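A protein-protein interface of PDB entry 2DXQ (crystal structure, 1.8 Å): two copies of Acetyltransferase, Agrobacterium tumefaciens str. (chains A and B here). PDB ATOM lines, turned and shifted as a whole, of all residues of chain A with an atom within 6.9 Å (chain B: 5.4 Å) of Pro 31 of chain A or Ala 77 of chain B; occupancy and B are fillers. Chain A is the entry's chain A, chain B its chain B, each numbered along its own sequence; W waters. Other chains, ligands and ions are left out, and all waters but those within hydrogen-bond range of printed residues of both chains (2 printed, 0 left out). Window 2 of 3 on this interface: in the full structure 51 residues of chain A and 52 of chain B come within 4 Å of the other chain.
Of the 11 printed residues of chain A, 5 touch a printed residue of chain B. Hydrophobic or aromatic side chains of chain A within 4 Å of the printed part of chain B: Pro 31, Leu 33 and Val 41. Among the printed residues, Asp or Glu carboxylates within 4 Å of a Lys or Arg side-chain nitrogen of the other chain: Asp 30 of chain A with Arg 76 of chain B.
NH1 of Arg 76 of chain B lies within salt-bridge range of OD1 of Asp 30 of chain A, 2.7 Å away.
Pro 31 of chain A touches just one residue of chain B: Ala 77 (3.8 Å). Printed residues of chain A within 4 Å of Leu 74 of chain B: Leu 33 and Val 41. Of the printed residues of chain A, Thr 75 of chain B touches Asn 27 and Asp 30. Of the printed residues of chain A, Ala 78 of chain B touches Leu 33. The nearest printed residue of chain A that does not touch Ala 77 of chain B is Asp 30 of chain A (4.6 Å). The nearest printed residue of chain B that does not touch Val 41 of chain A is Ala 78 of chain B (4.2 Å).
ND2 of Asn 27 of chain A touches CB of Thr 75 of chain B (3.6 Å). NH1 of Arg 76 of chain B touches CG of Asn 27 of chain A, 3.5 Å away. C of Thr 75 of chain B touches OD2 of Asp 30 of chain A (3.8 Å). Pro 31 of chain A touches Ala 77 of chain B (CG to CB, 3.8 Å). Leu 33 of chain A touches Leu 74 of chain B (CD1 to O, 3.5 Å). Ala 77 of chain B touches Leu 33 of chain A. N of Ala 78 of chain B touches CD1 of Leu 33 of chain A, at 3.8 Å. CG1 of Val 41 of chain A touches CD2 of Leu 74 of chain B, at 3.7 Å.
The side-chain amide nitrogen of Asn 27 of chain A is in hydrogen-bond range of the side-chain carboxylate of Asp 30 of chain A.
Water W2 lies within hydrogen-bond range of OG1 of Thr 75 of chain B (2.8 Å) and ND2 of Asn 27 of chain A (3.0 Å). Water W1 lies within hydrogen-bond range of O of Pro 31 of chain A and N of Ala 77 of chain B.
No position is printed for both chains. Of the 9 pairs that touch across the chains among the printed residues, none has its exchanged pair printed and touching as well.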
ATOM      1  N   GLN A  24      12.455 -19.501 -15.631  1.00  0.00           N
ATOM      2  CA  GLN A  24      12.155 -18.647 -16.781  1.00  0.00           C
ATOM      3  C   GLN A  24      11.088 -19.269 -17.691  1.00  0.00           C
ATOM      4  O   GLN A  24      10.250 -18.553 -18.258  1.00  0.00           O
ATOM      5  CB  GLN A  24      13.447 -18.291 -17.531  1.00  0.00           C
ATOM      6  CG  GLN A  24      14.259 -17.266 -16.710  1.00  0.00           C
ATOM      7  CD  GLN A  24      15.760 -17.291 -16.934  1.00  0.00           C
ATOM      8  OE1 GLN A  24      16.238 -17.735 -17.982  1.00  0.00           O
ATOM      9  NE2 GLN A  24      16.521 -16.781 -15.943  1.00  0.00           N
ATOM     10  N   ASN A  27       7.671 -18.777 -15.703  1.00  0.00           N
ATOM     11  CA  ASN A  27       7.152 -17.415 -15.797  1.00  0.00           C
ATOM     12  C   ASN A  27       7.917 -16.637 -16.868  1.00  0.00           C
ATOM     13  O   ASN A  27       8.883 -15.939 -16.555  1.00  0.00           O
ATOM     14  CB  ASN A  27       7.266 -16.694 -14.441  1.00  0.00           C
ATOM     15  CG  ASN A  27       6.530 -17.404 -13.297  1.00  0.00           C
ATOM     16  OD1 ASN A  27       5.450 -17.959 -13.465  1.00  0.00           O
ATOM     17  ND2 ASN A  27       7.116 -17.354 -12.116  1.00  0.00           N
ATOM     18  N   PRO A  28       7.506 -16.763 -18.147  1.00  0.00           N
ATOM     19  CA  PRO A  28       8.255 -16.107 -19.238  1.00  0.00           C
ATOM     20  C   PRO A  28       8.370 -14.575 -19.162  1.00  0.00           C
ATOM     21  O   PRO A  28       9.259 -14.008 -19.796  1.00  0.00           O
ATOM     22  CB  PRO A  28       7.522 -16.553 -20.515  1.00  0.00           C
ATOM     23  CG  PRO A  28       6.221 -17.115 -20.074  1.00  0.00           C
ATOM     24  CD  PRO A  28       6.356 -17.552 -18.644  1.00  0.00           C
ATOM     25  N   SER A  29       7.506 -13.923 -18.390  1.00  0.00           N
ATOM     26  CA  SER A  29       7.572 -12.461 -18.246  1.00  0.00           C
ATOM     27  C   SER A  29       8.457 -12.014 -17.063  1.00  0.00           C
ATOM     28  O   SER A  29       8.714 -10.812 -16.878  1.00  0.00           O
ATOM     29  CB  SER A  29       6.169 -11.871 -18.143  1.00  0.00           C
ATOM     30  OG  SER A  29       5.621 -12.099 -16.859  1.00  0.00           O
ATOM     31  N   ASP A  30       8.930 -12.971 -16.261  1.00  0.00           N
ATOM     32  CA  ASP A  30       9.837 -12.639 -15.156  1.00  0.00           C
ATOM     33  C   ASP A  30      11.168 -12.163 -15.704  1.00  0.00           C
ATOM     34  O   ASP A  30      11.598 -12.638 -16.757  1.00  0.00           O
ATOM     35  CB  ASP A  30      10.098 -13.860 -14.264  1.00  0.00           C
ATOM     36  CG  ASP A  30       9.088 -14.006 -13.139  1.00  0.00           C
ATOM     37  OD1 ASP A  30       8.227 -13.107 -12.916  1.00  0.00           O
ATOM     38  OD2 ASP A  30       9.177 -15.035 -12.445  1.00  0.00           O
ATOM     39  N   PRO A  31      11.849 -11.251 -14.969  1.00  0.00           N
ATOM     40  CA  PRO A  31      13.194 -10.843 -15.365  1.00  0.00           C
ATOM     41  C   PRO A  31      14.145 -12.029 -15.284  1.00  0.00           C
ATOM     42  O   PRO A  31      13.945 -12.930 -14.458  1.00  0.00           O
ATOM     43  CB  PRO A  31      13.575  -9.798 -14.313  1.00  0.00           C
ATOM     44  CG  PRO A  31      12.723 -10.075 -13.144  1.00  0.00           C
ATOM     45  CD  PRO A  31      11.416 -10.572 -13.735  1.00  0.00           C
ATOM     46  N   GLU A  32      15.153 -12.037 -16.142  1.00  0.00           N
ATOM     47  CA  GLU A  32      16.082 -13.166 -16.183  1.00  0.00           C
ATOM     48  C   GLU A  32      17.219 -12.884 -15.215  1.00  0.00           C
ATOM     49  O   GLU A  32      18.195 -12.224 -15.561  1.00  0.00           O
ATOM     50  CB  GLU A  32      16.560 -13.429 -17.618  1.00  0.00           C
ATOM     51  CG  GLU A  32      15.383 -13.675 -18.568  1.00  0.00           C
ATOM     52  CD  GLU A  32      15.794 -14.039 -19.991  1.00  0.00           C
ATOM     53  OE1 GLU A  32      16.979 -13.882 -20.359  1.00  0.00           O
ATOM     54  OE2 GLU A  32      14.907 -14.495 -20.744  1.00  0.00           O
ATOM     55  N   LEU A  33      17.045 -13.351 -13.977  1.00  0.00           N
ATOM     56  CA  LEU A  33      18.056 -13.205 -12.932  1.00  0.00           C
ATOM     57  C   LEU A  33      19.315 -13.948 -13.324  1.00  0.00           C
ATOM     58  O   LEU A  33      19.245 -15.064 -13.837  1.00  0.00           O
ATOM     59  CB  LEU A  33      17.555 -13.803 -11.611  1.00  0.00           C
ATOM     60  CG  LEU A  33      16.366 -13.146 -10.930  1.00  0.00           C
ATOM     61  CD1 LEU A  33      16.070 -13.909  -9.652  1.00  0.00           C
ATOM     62  CD2 LEU A  33      16.645 -11.684 -10.623  1.00  0.00           C
ATOM     63  N   THR A  34      20.469 -13.328 -13.094  1.00  0.00           N
ATOM     64  CA  THR A  34      21.730 -14.029 -13.308  1.00  0.00           C
ATOM     65  C   THR A  34      22.021 -14.921 -12.102  1.00  0.00           C
ATOM     66  O   THR A  34      21.426 -14.764 -11.034  1.00  0.00           O
ATOM     67  CB  THR A  34      22.880 -13.035 -13.489  1.00  0.00           C
ATOM     68  OG1 THR A  34      23.060 -12.311 -12.259  1.00  0.00           O
ATOM     69  CG2 THR A  34      22.542 -12.064 -14.611  1.00  0.00           C
ATOM     70  N   GLU A  37      22.975 -12.617  -9.272  1.00  0.00           N
ATOM     71  CA  GLU A  37      21.806 -11.956  -8.648  1.00  0.00           C
ATOM     72  C   GLU A  37      21.019 -12.913  -7.765  1.00  0.00           C
ATOM     73  O   GLU A  37      20.437 -12.508  -6.749  1.00  0.00           O
ATOM     74  CB  GLU A  37      20.870 -11.389  -9.719  1.00  0.00           C
ATOM     75  CG  GLU A  37      21.405 -10.109 -10.378  1.00  0.00           C
ATOM     76  CD  GLU A  37      20.615  -9.680 -11.592  1.00  0.00           C
ATOM     77  OE1 GLU A  37      19.973 -10.541 -12.249  1.00  0.00           O
ATOM     78  OE2 GLU A  37      20.664  -8.470 -11.926  1.00  0.00           O
ATOM     79  N   VAL A  41      19.751 -15.514  -2.331  1.00  0.00           N
ATOM     80  CA  VAL A  41      18.485 -16.212  -2.049  1.00  0.00           C
ATOM     81  C   VAL A  41      18.630 -17.730  -2.204  1.00  0.00           C
ATOM     82  O   VAL A  41      18.131 -18.490  -1.366  1.00  0.00           O
ATOM     83  CB  VAL A  41      17.299 -15.657  -2.883  1.00  0.00           C
ATOM     84  CG1 VAL A  41      16.059 -16.509  -2.663  1.00  0.00           C
ATOM     85  CG2 VAL A  41      16.995 -14.244  -2.449  1.00  0.00           C
ATOM     86  N   LEU B  74      12.960 -17.885  -5.760  1.00  0.00           N
ATOM     87  CA  LEU B  74      13.707 -17.348  -6.893  1.00  0.00           C
ATOM     88  C   LEU B  74      12.885 -16.789  -8.032  1.00  0.00           C
ATOM     89  O   LEU B  74      13.419 -16.043  -8.852  1.00  0.00           O
ATOM     90  CB  LEU B  74      14.675 -18.395  -7.446  1.00  0.00           C
ATOM     91  CG  LEU B  74      15.823 -18.788  -6.521  1.00  0.00           C
ATOM     92  CD1 LEU B  74      16.625 -19.862  -7.195  1.00  0.00           C
ATOM     93  CD2 LEU B  74      16.701 -17.578  -6.182  1.00  0.00           C
ATOM     94  N   THR B  75      11.602 -17.140  -8.108  1.00  0.00           N
ATOM     95  CA  THR B  75      10.749 -16.592  -9.156  1.00  0.00           C
ATOM     96  C   THR B  75      10.383 -15.156  -8.802  1.00  0.00           C
ATOM     97  O   THR B  75      10.658 -14.695  -7.685  1.00  0.00           O
ATOM     98  CB  THR B  75       9.455 -17.442  -9.354  1.00  0.00           C
ATOM     99  OG1 THR B  75       8.576 -17.242  -8.251  1.00  0.00           O
ATOM    100  CG2 THR B  75       9.795 -18.925  -9.478  1.00  0.00           C
ATOM    101  N   ARG B  76       9.745 -14.460  -9.746  1.00  0.00           N
ATOM    102  CA  ARG B  76       9.286 -13.080  -9.546  1.00  0.00           C
ATOM    103  C   ARG B  76      10.394 -12.199  -8.993  1.00  0.00           C
ATOM    104  O   ARG B  76      10.196 -11.518  -7.995  1.00  0.00           O
ATOM    105  CB  ARG B  76       8.046 -12.995  -8.631  1.00  0.00           C
ATOM    106  CG  ARG B  76       6.690 -13.108  -9.359  1.00  0.00           C
ATOM    107  CD  ARG B  76       6.531 -14.471  -9.994  1.00  0.00           C
ATOM    108  NE  ARG B  76       5.183 -14.687 -10.549  1.00  0.00           N
ATOM    109  CZ  ARG B  76       4.839 -14.480 -11.817  1.00  0.00           C
ATOM    110  NH1 ARG B  76       5.726 -14.053 -12.704  1.00  0.00           N
ATOM    111  NH2 ARG B  76       3.591 -14.731 -12.215  1.00  0.00           N
ATOM    112  N   ALA B  77      11.546 -12.224  -9.657  1.00  0.00           N
ATOM    113  CA  ALA B  77      12.695 -11.409  -9.271  1.00  0.00           C
ATOM    114  C   ALA B  77      13.216 -11.756  -7.872  1.00  0.00           C
ATOM    115  O   ALA B  77      13.735 -10.894  -7.141  1.00  0.00           O
ATOM    116  CB  ALA B  77      12.341  -9.908  -9.385  1.00  0.00           C
ATOM    117  N   ALA B  78      13.089 -13.037  -7.512  1.00  0.00           N
ATOM    118  CA  ALA B  78      13.481 -13.563  -6.215  1.00  0.00           C
ATOM    119  C   ALA B  78      12.776 -12.902  -5.017  1.00  0.00           C
ATOM    120  O   ALA B  78      13.355 -12.776  -3.945  1.00  0.00           O
ATOM    121  CB  ALA B  78      15.013 -13.566  -6.045  1.00  0.00           C
ATOM    122  N   ARG B  79      11.519 -12.513  -5.210  1.00  0.00           N
ATOM    123  CA  ARG B  79      10.688 -12.027  -4.098  1.00  0.00           C
ATOM    124  C   ARG B  79      10.108 -13.193  -3.328  1.00  0.00           C
ATOM    125  O   ARG B  79       9.705 -14.194  -3.944  1.00  0.00           O
ATOM    126  CB  ARG B  79       9.561 -11.117  -4.588  1.00  0.00           C
ATOM    127  CG  ARG B  79      10.048  -9.728  -5.005  1.00  0.00           C
ATOM    128  CD  ARG B  79       8.904  -8.928  -5.567  1.00  0.00           C
ATOM    129  NE  ARG B  79       8.041  -8.379  -4.519  1.00  0.00           N
ATOM    130  CZ  ARG B  79       6.934  -7.677  -4.756  1.00  0.00           C
ATOM    131  NH1 ARG B  79       6.534  -7.445  -6.002  1.00  0.00           N
ATOM    132  NH2 ARG B  79       6.224  -7.202  -3.745  1.00  0.00           N
HETATM  133  O   HOH W   1      12.763 -13.515 -11.986  1.00  0.00           O
HETATM  134  O   HOH W   2       6.294 -18.400  -9.388  1.00  0.00           O
